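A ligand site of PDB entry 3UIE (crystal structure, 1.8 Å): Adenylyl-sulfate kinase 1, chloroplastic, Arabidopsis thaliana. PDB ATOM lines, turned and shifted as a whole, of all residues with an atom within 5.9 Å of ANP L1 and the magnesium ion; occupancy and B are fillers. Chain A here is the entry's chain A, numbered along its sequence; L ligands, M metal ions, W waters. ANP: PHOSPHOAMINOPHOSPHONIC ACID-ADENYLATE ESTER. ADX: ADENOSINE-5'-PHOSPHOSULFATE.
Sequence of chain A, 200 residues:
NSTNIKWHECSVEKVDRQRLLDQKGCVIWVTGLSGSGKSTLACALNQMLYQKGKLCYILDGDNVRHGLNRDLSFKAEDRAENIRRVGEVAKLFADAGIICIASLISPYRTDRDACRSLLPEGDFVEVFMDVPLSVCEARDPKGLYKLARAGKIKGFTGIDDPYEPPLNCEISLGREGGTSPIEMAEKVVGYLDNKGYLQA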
ATOM      1  N   GLY A  32     -20.607 -10.583  33.551  1.00  0.00           N
ATOM      2  CA  GLY A  32     -21.979 -10.092  33.627  1.00  0.00           C
ATOM      3  C   GLY A  32     -22.790 -10.674  32.485  1.00  0.00           C
ATOM      4  O   GLY A  32     -22.227 -11.232  31.541  1.00  0.00           O
ATOM      5  N   LEU A  33     -24.105 -10.552  32.599  1.00  0.00           N
ATOM      6  CA  LEU A  33     -25.021 -11.019  31.548  1.00  0.00           C
ATOM      7  C   LEU A  33     -24.673 -10.433  30.198  1.00  0.00           C
ATOM      8  O   LEU A  33     -24.034  -9.385  30.120  1.00  0.00           O
ATOM      9  CB  LEU A  33     -26.457 -10.588  31.918  1.00  0.00           C
ATOM     10  CG  LEU A  33     -27.105 -11.255  33.124  1.00  0.00           C
ATOM     11  CD1 LEU A  33     -28.450 -10.578  33.426  1.00  0.00           C
ATOM     12  CD2 LEU A  33     -27.291 -12.746  32.829  1.00  0.00           C
ATOM     13  N   SER A  34     -25.094 -11.100  29.123  1.00  0.00           N
ATOM     14  CA  SER A  34     -25.097 -10.497  27.809  1.00  0.00           C
ATOM     15  C   SER A  34     -25.845  -9.165  27.870  1.00  0.00           C
ATOM     16  O   SER A  34     -26.938  -9.085  28.442  1.00  0.00           O
ATOM     17  CB  SER A  34     -25.777 -11.420  26.791  1.00  0.00           C
ATOM     18  OG  SER A  34     -25.607 -10.947  25.481  1.00  0.00           O
ATOM     19  N   GLY A  35     -25.247  -8.126  27.306  1.00  0.00           N
ATOM     20  CA  GLY A  35     -25.883  -6.818  27.253  1.00  0.00           C
ATOM     21  C   GLY A  35     -25.663  -5.958  28.492  1.00  0.00           C
ATOM     22  O   GLY A  35     -26.181  -4.845  28.563  1.00  0.00           O
ATOM     23  N   SER A  36     -24.904  -6.472  29.456  1.00  0.00           N
ATOM     24  CA  SER A  36     -24.690  -5.750  30.718  1.00  0.00           C
ATOM     25  C   SER A  36     -23.691  -4.605  30.577  1.00  0.00           C
ATOM     26  O   SER A  36     -23.568  -3.761  31.460  1.00  0.00           O
ATOM     27  CB  SER A  36     -24.253  -6.704  31.838  1.00  0.00           C
ATOM     28  OG  SER A  36     -23.064  -7.393  31.496  1.00  0.00           O
ATOM     29  N   GLY A  37     -22.986  -4.587  29.454  1.00  0.00           N
ATOM     30  CA  GLY A  37     -22.056  -3.520  29.140  1.00  0.00           C
ATOM     31  C   GLY A  37     -20.577  -3.826  29.416  1.00  0.00           C
ATOM     32  O   GLY A  37     -19.783  -2.910  29.613  1.00  0.00           O
ATOM     33  N   LYS A  38     -20.213  -5.105  29.418  1.00  0.00           N
ATOM     34  CA  LYS A  38     -18.828  -5.507  29.676  1.00  0.00           C
ATOM     35  C   LYS A  38     -17.844  -4.942  28.644  1.00  0.00           C
ATOM     36  O   LYS A  38     -16.807  -4.374  29.005  1.00  0.00           O
ATOM     37  CB  LYS A  38     -18.717  -7.044  29.729  1.00  0.00           C
ATOM     38  CG  LYS A  38     -19.559  -7.716  30.812  1.00  0.00           C
ATOM     39  CD  LYS A  38     -19.423  -9.242  30.673  1.00  0.00           C
ATOM     40  CE  LYS A  38     -19.822  -9.755  29.283  1.00  0.00           C
ATOM     41  NZ  LYS A  38     -21.312  -9.677  29.053  1.00  0.00           N
ATOM     42  N   SER A  39     -18.161  -5.102  27.367  1.00  0.00           N
ATOM     43  CA  SER A  39     -17.251  -4.652  26.299  1.00  0.00           C
ATOM     44  C   SER A  39     -17.145  -3.134  26.265  1.00  0.00           C
ATOM     45  O   SER A  39     -16.072  -2.565  26.002  1.00  0.00           O
ATOM     46  CB  SER A  39     -17.696  -5.213  24.940  1.00  0.00           C
ATOM     47  OG  SER A  39     -17.565  -6.628  24.945  1.00  0.00           O
ATOM     48  N   THR A  40     -18.266  -2.481  26.513  1.00  0.00           N
ATOM     49  CA  THR A  40     -18.290  -1.034  26.515  1.00  0.00           C
ATOM     50  C   THR A  40     -17.401  -0.481  27.637  1.00  0.00           C
ATOM     51  O   THR A  40     -16.624   0.473  27.433  1.00  0.00           O
ATOM     52  CB  THR A  40     -19.716  -0.522  26.661  1.00  0.00           C
ATOM     53  OG1 THR A  40     -20.476  -0.950  25.524  1.00  0.00           O
ATOM     54  CG2 THR A  40     -19.711   0.980  26.735  1.00  0.00           C
ATOM     55  N   LEU A  41     -17.505  -1.086  28.804  1.00  0.00           N
ATOM     56  CA  LEU A  41     -16.638  -0.738  29.918  1.00  0.00           C
ATOM     57  C   LEU A  41     -15.173  -1.066  29.604  1.00  0.00           C
ATOM     58  O   LEU A  41     -14.271  -0.263  29.868  1.00  0.00           O
ATOM     59  CB  LEU A  41     -17.074  -1.473  31.192  1.00  0.00           C
ATOM     60  CG  LEU A  41     -16.016  -1.307  32.287  1.00  0.00           C
ATOM     61  CD1 LEU A  41     -16.012   0.128  32.809  1.00  0.00           C
ATOM     62  CD2 LEU A  41     -16.231  -2.303  33.394  1.00  0.00           C
ATOM     63  N   ASP A  60     -11.684 -10.267  24.757  1.00  0.00           N
ATOM     64  CA  ASP A  60     -13.132 -10.272  24.728  1.00  0.00           C
ATOM     65  C   ASP A  60     -13.669 -11.621  24.287  1.00  0.00           C
ATOM     66  O   ASP A  60     -13.195 -12.216  23.298  1.00  0.00           O
ATOM     67  CB  ASP A  60     -13.642  -9.176  23.796  1.00  0.00           C
ATOM     68  CG  ASP A  60     -15.148  -9.023  23.857  1.00  0.00           C
ATOM     69  OD1 ASP A  60     -15.633  -8.345  24.787  1.00  0.00           O
ATOM     70  OD2 ASP A  60     -15.839  -9.592  22.998  1.00  0.00           O
ATOM     71  N   ASP A  62     -16.237 -12.687  22.707  1.00  0.00           N
ATOM     72  CA  ASP A  62     -16.599 -12.828  21.298  1.00  0.00           C
ATOM     73  C   ASP A  62     -15.348 -12.957  20.421  1.00  0.00           C
ATOM     74  O   ASP A  62     -15.218 -13.905  19.636  1.00  0.00           O
ATOM     75  CB  ASP A  62     -17.476 -11.659  20.840  1.00  0.00           C
ATOM     76  CG  ASP A  62     -18.094 -11.894  19.470  1.00  0.00           C
ATOM     77  OD1 ASP A  62     -18.500 -13.047  19.189  1.00  0.00           O
ATOM     78  OD2 ASP A  62     -18.177 -10.934  18.675  1.00  0.00           O
ATOM     79  N   SER A 103     -13.189  -9.694  29.153  1.00  0.00           N
ATOM     80  CA  SER A 103     -14.595  -9.327  29.084  1.00  0.00           C
ATOM     81  C   SER A 103     -15.401 -10.490  28.522  1.00  0.00           C
ATOM     82  O   SER A 103     -15.529 -10.612  27.315  1.00  0.00           O
ATOM     83  CB  SER A 103     -14.772  -8.088  28.211  1.00  0.00           C
ATOM     84  OG  SER A 103     -16.138  -7.806  27.913  1.00  0.00           O
ATOM     85  N   LEU A 104     -15.903 -11.356  29.394  1.00  0.00           N
ATOM     86  CA  LEU A 104     -16.594 -12.581  29.005  1.00  0.00           C
ATOM     87  C   LEU A 104     -17.790 -12.706  29.922  1.00  0.00           C
ATOM     88  O   LEU A 104     -17.701 -12.315  31.083  1.00  0.00           O
ATOM     89  CB  LEU A 104     -15.704 -13.792  29.277  1.00  0.00           C
ATOM     90  CG  LEU A 104     -14.756 -14.503  28.327  1.00  0.00           C
ATOM     91  CD1 LEU A 104     -13.563 -13.643  27.966  1.00  0.00           C
ATOM     92  CD2 LEU A 104     -14.303 -15.789  29.011  1.00  0.00           C
ATOM     93  N   ILE A 105     -18.896 -13.253  29.424  1.00  0.00           N
ATOM     94  CA  ILE A 105     -20.043 -13.502  30.300  1.00  0.00           C
ATOM     95  C   ILE A 105     -19.600 -14.289  31.529  1.00  0.00           C
ATOM     96  O   ILE A 105     -19.959 -13.947  32.657  1.00  0.00           O
ATOM     97  CB  ILE A 105     -21.192 -14.248  29.568  1.00  0.00           C
ATOM     98  CG1 ILE A 105     -21.742 -13.381  28.440  1.00  0.00           C
ATOM     99  CG2 ILE A 105     -22.311 -14.619  30.554  1.00  0.00           C
ATOM    100  CD1 ILE A 105     -22.825 -14.070  27.599  1.00  0.00           C
ATOM    101  N   MET A 129     -20.533  -6.422  36.288  1.00  0.00           N
ATOM    102  CA  MET A 129     -21.495  -5.531  35.678  1.00  0.00           C
ATOM    103  C   MET A 129     -22.882  -5.861  36.236  1.00  0.00           C
ATOM    104  O   MET A 129     -23.602  -6.719  35.702  1.00  0.00           O
ATOM    105  CB  MET A 129     -21.483  -5.656  34.151  1.00  0.00           C
ATOM    106  CG  MET A 129     -20.092  -5.420  33.508  1.00  0.00           C
ATOM    107  SD  MET A 129     -19.276  -3.908  34.077  1.00  0.00           S
ATOM    108  CE  MET A 129     -20.312  -2.670  33.305  1.00  0.00           C
ATOM    109  N   ARG A 139     -32.125  -3.621  26.410  1.00  0.00           N
ATOM    110  CA  ARG A 139     -31.048  -3.225  25.500  1.00  0.00           C
ATOM    111  C   ARG A 139     -30.987  -4.188  24.315  1.00  0.00           C
ATOM    112  O   ARG A 139     -31.184  -3.788  23.172  1.00  0.00           O
ATOM    113  CB  ARG A 139     -29.695  -3.198  26.229  1.00  0.00           C
ATOM    114  CG  ARG A 139     -29.592  -2.117  27.311  1.00  0.00           C
ATOM    115  CD  ARG A 139     -28.334  -2.302  28.134  1.00  0.00           C
ATOM    116  NE  ARG A 139     -28.167  -1.272  29.164  1.00  0.00           N
ATOM    117  CZ  ARG A 139     -27.109  -1.196  29.974  1.00  0.00           C
ATOM    118  NH1 ARG A 139     -26.141  -2.104  29.866  1.00  0.00           N
ATOM    119  NH2 ARG A 139     -27.018  -0.235  30.875  1.00  0.00           N
ATOM    120  N   PRO A 141     -28.909  -5.501  22.302  1.00  0.00           N
ATOM    121  CA  PRO A 141     -28.294  -4.843  21.138  1.00  0.00           C
ATOM    122  C   PRO A 141     -28.204  -5.761  19.923  1.00  0.00           C
ATOM    123  O   PRO A 141     -28.316  -5.283  18.795  1.00  0.00           O
ATOM    124  CB  PRO A 141     -26.877  -4.512  21.630  1.00  0.00           C
ATOM    125  CG  PRO A 141     -26.910  -4.654  23.090  1.00  0.00           C
ATOM    126  CD  PRO A 141     -27.958  -5.657  23.411  1.00  0.00           C
ATOM    127  N   LYS A 142     -27.997  -7.052  20.158  1.00  0.00           N
ATOM    128  CA  LYS A 142     -27.773  -8.004  19.083  1.00  0.00           C
ATOM    129  C   LYS A 142     -28.999  -8.867  18.794  1.00  0.00           C
ATOM    130  O   LYS A 142     -28.957  -9.733  17.917  1.00  0.00           O
ATOM    131  CB  LYS A 142     -26.571  -8.900  19.412  1.00  0.00           C
ATOM    132  CG  LYS A 142     -25.308  -8.135  19.772  1.00  0.00           C
ATOM    133  CD  LYS A 142     -24.237  -9.068  20.336  1.00  0.00           C
ATOM    134  CE  LYS A 142     -23.117  -8.275  21.005  1.00  0.00           C
ATOM    135  NZ  LYS A 142     -22.052  -9.160  21.576  1.00  0.00           N
ATOM    136  N   LEU A 144     -30.274 -11.085  20.734  1.00  0.00           N
ATOM    137  CA  LEU A 144     -30.055 -12.438  21.231  1.00  0.00           C
ATOM    138  C   LEU A 144     -31.116 -12.898  22.224  1.00  0.00           C
ATOM    139  O   LEU A 144     -31.516 -14.063  22.198  1.00  0.00           O
ATOM    140  CB  LEU A 144     -28.679 -12.562  21.880  1.00  0.00           C
ATOM    141  CG  LEU A 144     -27.501 -12.434  20.921  1.00  0.00           C
ATOM    142  CD1 LEU A 144     -26.218 -12.399  21.711  1.00  0.00           C
ATOM    143  CD2 LEU A 144     -27.509 -13.567  19.928  1.00  0.00           C
ATOM    144  N   THR A 179     -25.283   5.572  34.899  1.00  0.00           N
ATOM    145  CA  THR A 179     -23.856   5.685  35.166  1.00  0.00           C
ATOM    146  C   THR A 179     -23.125   5.369  33.851  1.00  0.00           C
ATOM    147  O   THR A 179     -23.279   4.300  33.258  1.00  0.00           O
ATOM    148  CB  THR A 179     -23.374   4.805  36.323  1.00  0.00           C
ATOM    149  OG1 THR A 179     -22.135   5.313  36.832  1.00  0.00           O
ATOM    150  CG2 THR A 179     -23.191   3.372  35.881  1.00  0.00           C
ATOM    151  N   SER A 180     -22.365   6.330  33.384  1.00  0.00           N
ATOM    152  CA  SER A 180     -21.829   6.274  32.035  1.00  0.00           C
ATOM    153  C   SER A 180     -20.613   5.350  31.980  1.00  0.00           C
ATOM    154  O   SER A 180     -19.950   5.111  32.995  1.00  0.00           O
ATOM    155  CB  SER A 180     -21.472   7.681  31.604  1.00  0.00           C
ATOM    156  OG  SER A 180     -20.326   8.122  32.321  1.00  0.00           O
ATOM    157  N   PRO A 181     -20.308   4.815  30.791  1.00  0.00           N
ATOM    158  CA  PRO A 181     -19.100   3.995  30.673  1.00  0.00           C
ATOM    159  C   PRO A 181     -17.864   4.763  31.127  1.00  0.00           C
ATOM    160  O   PRO A 181     -16.982   4.200  31.759  1.00  0.00           O
ATOM    161  CB  PRO A 181     -19.042   3.691  29.183  1.00  0.00           C
ATOM    162  CG  PRO A 181     -20.480   3.734  28.732  1.00  0.00           C
ATOM    163  CD  PRO A 181     -21.099   4.831  29.549  1.00  0.00           C
ATOM    164  N   MET A 184     -17.802   4.927  34.859  1.00  0.00           N
ATOM    165  CA  MET A 184     -17.446   3.599  35.377  1.00  0.00           C
ATOM    166  C   MET A 184     -15.957   3.285  35.208  1.00  0.00           C
ATOM    167  O   MET A 184     -15.347   2.701  36.103  1.00  0.00           O
ATOM    168  CB  MET A 184     -18.308   2.510  34.749  1.00  0.00           C
ATOM    169  CG  MET A 184     -19.740   2.546  35.240  1.00  0.00           C
ATOM    170  SD  MET A 184     -20.706   1.156  34.623  1.00  0.00           S
ATOM    171  CE  MET A 184     -20.481   1.307  32.892  1.00  0.00           C
HETATM  172  PG  ANP L   1     -22.082  -9.464  25.415  1.00  0.00           P
HETATM  173  O1G ANP L   1     -23.222 -10.212  24.560  1.00  0.00           O
HETATM  174  O2G ANP L   1     -20.912  -9.273  24.444  1.00  0.00           O
HETATM  175  O3G ANP L   1     -21.692 -10.308  26.595  1.00  0.00           O
HETATM  176  PB  ANP L   1     -21.750  -6.907  26.817  1.00  0.00           P
HETATM  177  O1B ANP L   1     -20.354  -6.626  26.151  1.00  0.00           O
HETATM  178  O2B ANP L   1     -21.802  -7.173  28.338  1.00  0.00           O
HETATM  179  N3B ANP L   1     -22.647  -7.914  25.773  1.00  0.00           N
HETATM  180  PA  ANP L   1     -22.035  -4.315  25.507  1.00  0.00           P
HETATM  181  O1A ANP L   1     -21.929  -4.769  24.087  1.00  0.00           O
HETATM  182  O2A ANP L   1     -20.800  -3.633  26.013  1.00  0.00           O
HETATM  183  O3A ANP L   1     -22.505  -5.542  26.368  1.00  0.00           O
HETATM  184  O5' ANP L   1     -23.250  -3.326  25.685  1.00  0.00           O
HETATM  185  C5' ANP L   1     -24.545  -3.644  25.284  1.00  0.00           C
HETATM  186  C4' ANP L   1     -25.350  -2.520  24.960  1.00  0.00           C
HETATM  187  O4' ANP L   1     -25.618  -1.719  26.150  1.00  0.00           O
HETATM  188  C3' ANP L   1     -24.583  -1.688  24.031  1.00  0.00           C
HETATM  189  O3' ANP L   1     -25.373  -1.376  22.896  1.00  0.00           O
HETATM  190  C2' ANP L   1     -24.229  -0.471  24.760  1.00  0.00           C
HETATM  191  O2' ANP L   1     -24.474   0.679  23.991  1.00  0.00           O
HETATM  192  C1' ANP L   1     -25.113  -0.445  25.952  1.00  0.00           C
HETATM  193  N9  ANP L   1     -24.366   0.044  27.112  1.00  0.00           N
HETATM  194  C8  ANP L   1     -23.124  -0.367  27.431  1.00  0.00           C
HETATM  195  N7  ANP L   1     -22.759   0.281  28.534  1.00  0.00           N
HETATM  196  C5  ANP L   1     -23.760   1.105  28.903  1.00  0.00           C
HETATM  197  C6  ANP L   1     -23.902   2.004  29.953  1.00  0.00           C
HETATM  198  N6  ANP L   1     -22.818   2.173  30.912  1.00  0.00           N
HETATM  199  N1  ANP L   1     -25.048   2.688  30.056  1.00  0.00           N
HETATM  200  C2  ANP L   1     -26.038   2.518  29.158  1.00  0.00           C
HETATM  201  N3  ANP L   1     -25.931   1.680  28.140  1.00  0.00           N
HETATM  202  C4  ANP L   1     -24.798   0.952  27.988  1.00  0.00           C
HETATM  203  SB  ADX L   2     -19.095 -17.432  28.026  1.00  0.00           S
HETATM  204  O1B ADX L   2     -18.471 -18.586  27.452  1.00  0.00           O
HETATM  205  O2B ADX L   2     -20.268 -17.861  28.806  1.00  0.00           O
HETATM  206  O3B ADX L   2     -18.172 -16.709  28.928  1.00  0.00           O
HETATM  207  PA  ADX L   2     -18.721 -15.517  26.038  1.00  0.00           P
HETATM  208  O1A ADX L   2     -17.417 -16.162  25.656  1.00  0.00           O
HETATM  209  O2A ADX L   2     -18.522 -14.145  26.666  1.00  0.00           O
HETATM  210  O3A ADX L   2     -19.594 -16.495  26.942  1.00  0.00           O
HETATM  211  O5' ADX L   2     -19.560 -15.362  24.717  1.00  0.00           O
HETATM  212  C5' ADX L   2     -20.710 -14.559  24.716  1.00  0.00           C
HETATM  213  C4' ADX L   2     -21.109 -14.041  23.432  1.00  0.00           C
HETATM  214  O4' ADX L   2     -21.488 -15.116  22.590  1.00  0.00           O
HETATM  215  C3' ADX L   2     -22.299 -13.170  23.614  1.00  0.00           C
HETATM  216  O3' ADX L   2     -22.007 -11.912  23.100  1.00  0.00           O
HETATM  217  C2' ADX L   2     -23.313 -13.706  22.807  1.00  0.00           C
HETATM  218  O2' ADX L   2     -23.494 -12.790  21.781  1.00  0.00           O
HETATM  219  C1' ADX L   2     -22.807 -14.949  22.181  1.00  0.00           C
HETATM  220  N9  ADX L   2     -23.660 -16.076  22.455  1.00  0.00           N
HETATM  221  C8  ADX L   2     -24.070 -17.001  21.557  1.00  0.00           C
HETATM  222  N7  ADX L   2     -24.783 -17.941  22.196  1.00  0.00           N
HETATM  223  C5  ADX L   2     -24.815 -17.629  23.508  1.00  0.00           C
HETATM  224  C6  ADX L   2     -25.405 -18.216  24.645  1.00  0.00           C
HETATM  225  N6  ADX L   2     -26.132 -19.431  24.523  1.00  0.00           N
HETATM  226  N1  ADX L   2     -25.264 -17.620  25.862  1.00  0.00           N
HETATM  227  C2  ADX L   2     -24.568 -16.479  25.982  1.00  0.00           C
HETATM  228  N3  ADX L   2     -23.995 -15.891  24.910  1.00  0.00           N
HETATM  229  C4  ADX L   2     -24.102 -16.435  23.677  1.00  0.00           C
HETATM  230 MG    MG M   1     -19.384  -7.889  24.655  1.00  0.00          MG
HETATM  231  O   HOH W   1     -20.113  -6.627  23.268  1.00  0.00           O
HETATM  232  O   HOH W   2     -22.935   3.223  25.513  1.00  0.00           O
HETATM  233  O   HOH W   3     -20.725  -0.452  30.330  1.00  0.00           O
HETATM  234  O   HOH W   4     -19.196 -11.437  26.137  1.00  0.00           O
HETATM  235  O   HOH W   5     -18.371  -8.838  23.124  1.00  0.00           O
HETATM  236  O   HOH W   6     -24.701  -7.183  23.806  1.00  0.00           O
HETATM  237  O   HOH W   7     -18.157  -9.174  26.056  1.00  0.00           O
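The magnesium ion is bound by water W1, water W5, O2G of ANP L1, O1B of ANP L1, OG of Ser 39 and water W7.
The backbone NH of Ser 39 lies within hydrogen-bond range of an oxygen (O2A) of ANP L1, 3.3 Å away.
N of Lys 38 lies within hydrogen-bond range of O2B of ANP L1, 2.8 Å away.
NZ of Lys 38 is in salt-bridge range of O3G of ANP L1, at 2.6 Å.
O1G of ANP L1 lies within hydrogen-bond range of OG of Ser 34 (2.7 Å).
N of Thr 40 lies within hydrogen-bond range of O2A of ANP L1.
An oxygen (O2A) of ANP L1 is in hydrogen-bond range of the side-chain hydroxyl of Thr 40.
An oxygen (O2B) of ANP L1 sits at hydrogen-bond distance from the backbone NH of Gly 37 (3.1 Å).
NZ of Lys 142 lies within salt-bridge range of O1G of ANP L1 (3.4 Å).
A nitrogen (N6) of ANP L1 sits at hydrogen-bond distance from the backbone carbonyl oxygen (O) of Thr 179 (3.2 Å).
The backbone NH (N) of Ser 36 is in hydrogen-bond range of an oxygen (O2B) of ANP L1 (3.4 Å).
The side-chain hydroxyl (OG) of Ser 36 lies within hydrogen-bond range of an oxygen (O2B) of ANP L1, 3.4 Å away.
The side-chain amino group (NZ) of Lys 142 sits at hydrogen-bond distance from an oxygen (O3') of ADX L2, at 3.1 Å.
N of Ile 105 sits at hydrogen-bond distance from O2A of ADX L2 (2.9 Å).
The backbone NH (N) of Gly 35 sits close to a nitrogen (N3B) of ANP L1 (3.0 Å).
Residues that only touch ANP L1: Leu 33 (3.6 Å), Ile 105 (3.6 Å), Arg 139 (3.4 Å), Pro 141 (3.2 Å), Pro 181 (3.4 Å) and Met 184 (3.2 Å).
Within 4 Å of ANP L1: Leu 33, Ser 34, Gly 35, Ser 36, Gly 37, Lys 38, Ser 39, Thr 40, Ile 105, Arg 139, Pro 141, Lys 142, Thr 179, Pro 181 and Met 184.
The nearest printed residue that does not touch ANP L1 is Ser 180 (4.01 Å).
Water W7 lies within hydrogen-bond range of OD1 of Asp 60 (2.9 Å) and OG of Ser 103 (3.1 Å).
Water W4 bridges O3G of ANP L1 (2.8 Å) and O2A of ADX L2 (2.8 Å).
Water W3 lies within hydrogen-bond range of O of Gly 37 (2.7 Å) and N7 of ANP L1 (2.8 Å).
An oxygen (O1G) of ANP L1 is in hydrogen-bond range of an oxygen (O3') of ADX L2.
Residues that only touch the magnesium ion: Asp 60 (3.8 Å).
Two residues have an atom within 4 Å of the magnesium ion: Ser 39 and Asp 60.
The side-chain carboxylate (OD1) of Asp 60 sits close to the side-chain hydroxyl (OG) of Ser 39 (2.6 Å).
The backbone NH (N) of Ser 39 is in hydrogen-bond range of the side-chain hydroxyl (OG) of Ser 103 (3.4 Å).
NZ of Lys 38 is in hydrogen-bond range of O of Leu 33 (2.9 Å).
The backbone carbonyl oxygen (O) of Gly 35 is in hydrogen-bond range of the guanidinium group (NH1) of Arg 139, at 3.0 Å.
The backbone carbonyl oxygen (O) of Ser 36 sits at hydrogen-bond distance from the guanidinium group (NH1) of Arg 139 (3.5 Å).
The backbone carbonyl oxygen (O) of Leu 33 lies within hydrogen-bond range of the side-chain hydroxyl (OG) of Ser 36.
The side-chain hydroxyl of Ser 103 lies within hydrogen-bond range of the side-chain carboxylate of Asp 60 (3.2 Å).
OD2 of Asp 60 lies within hydrogen-bond range of N of Asp 62 (3.1 Å).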
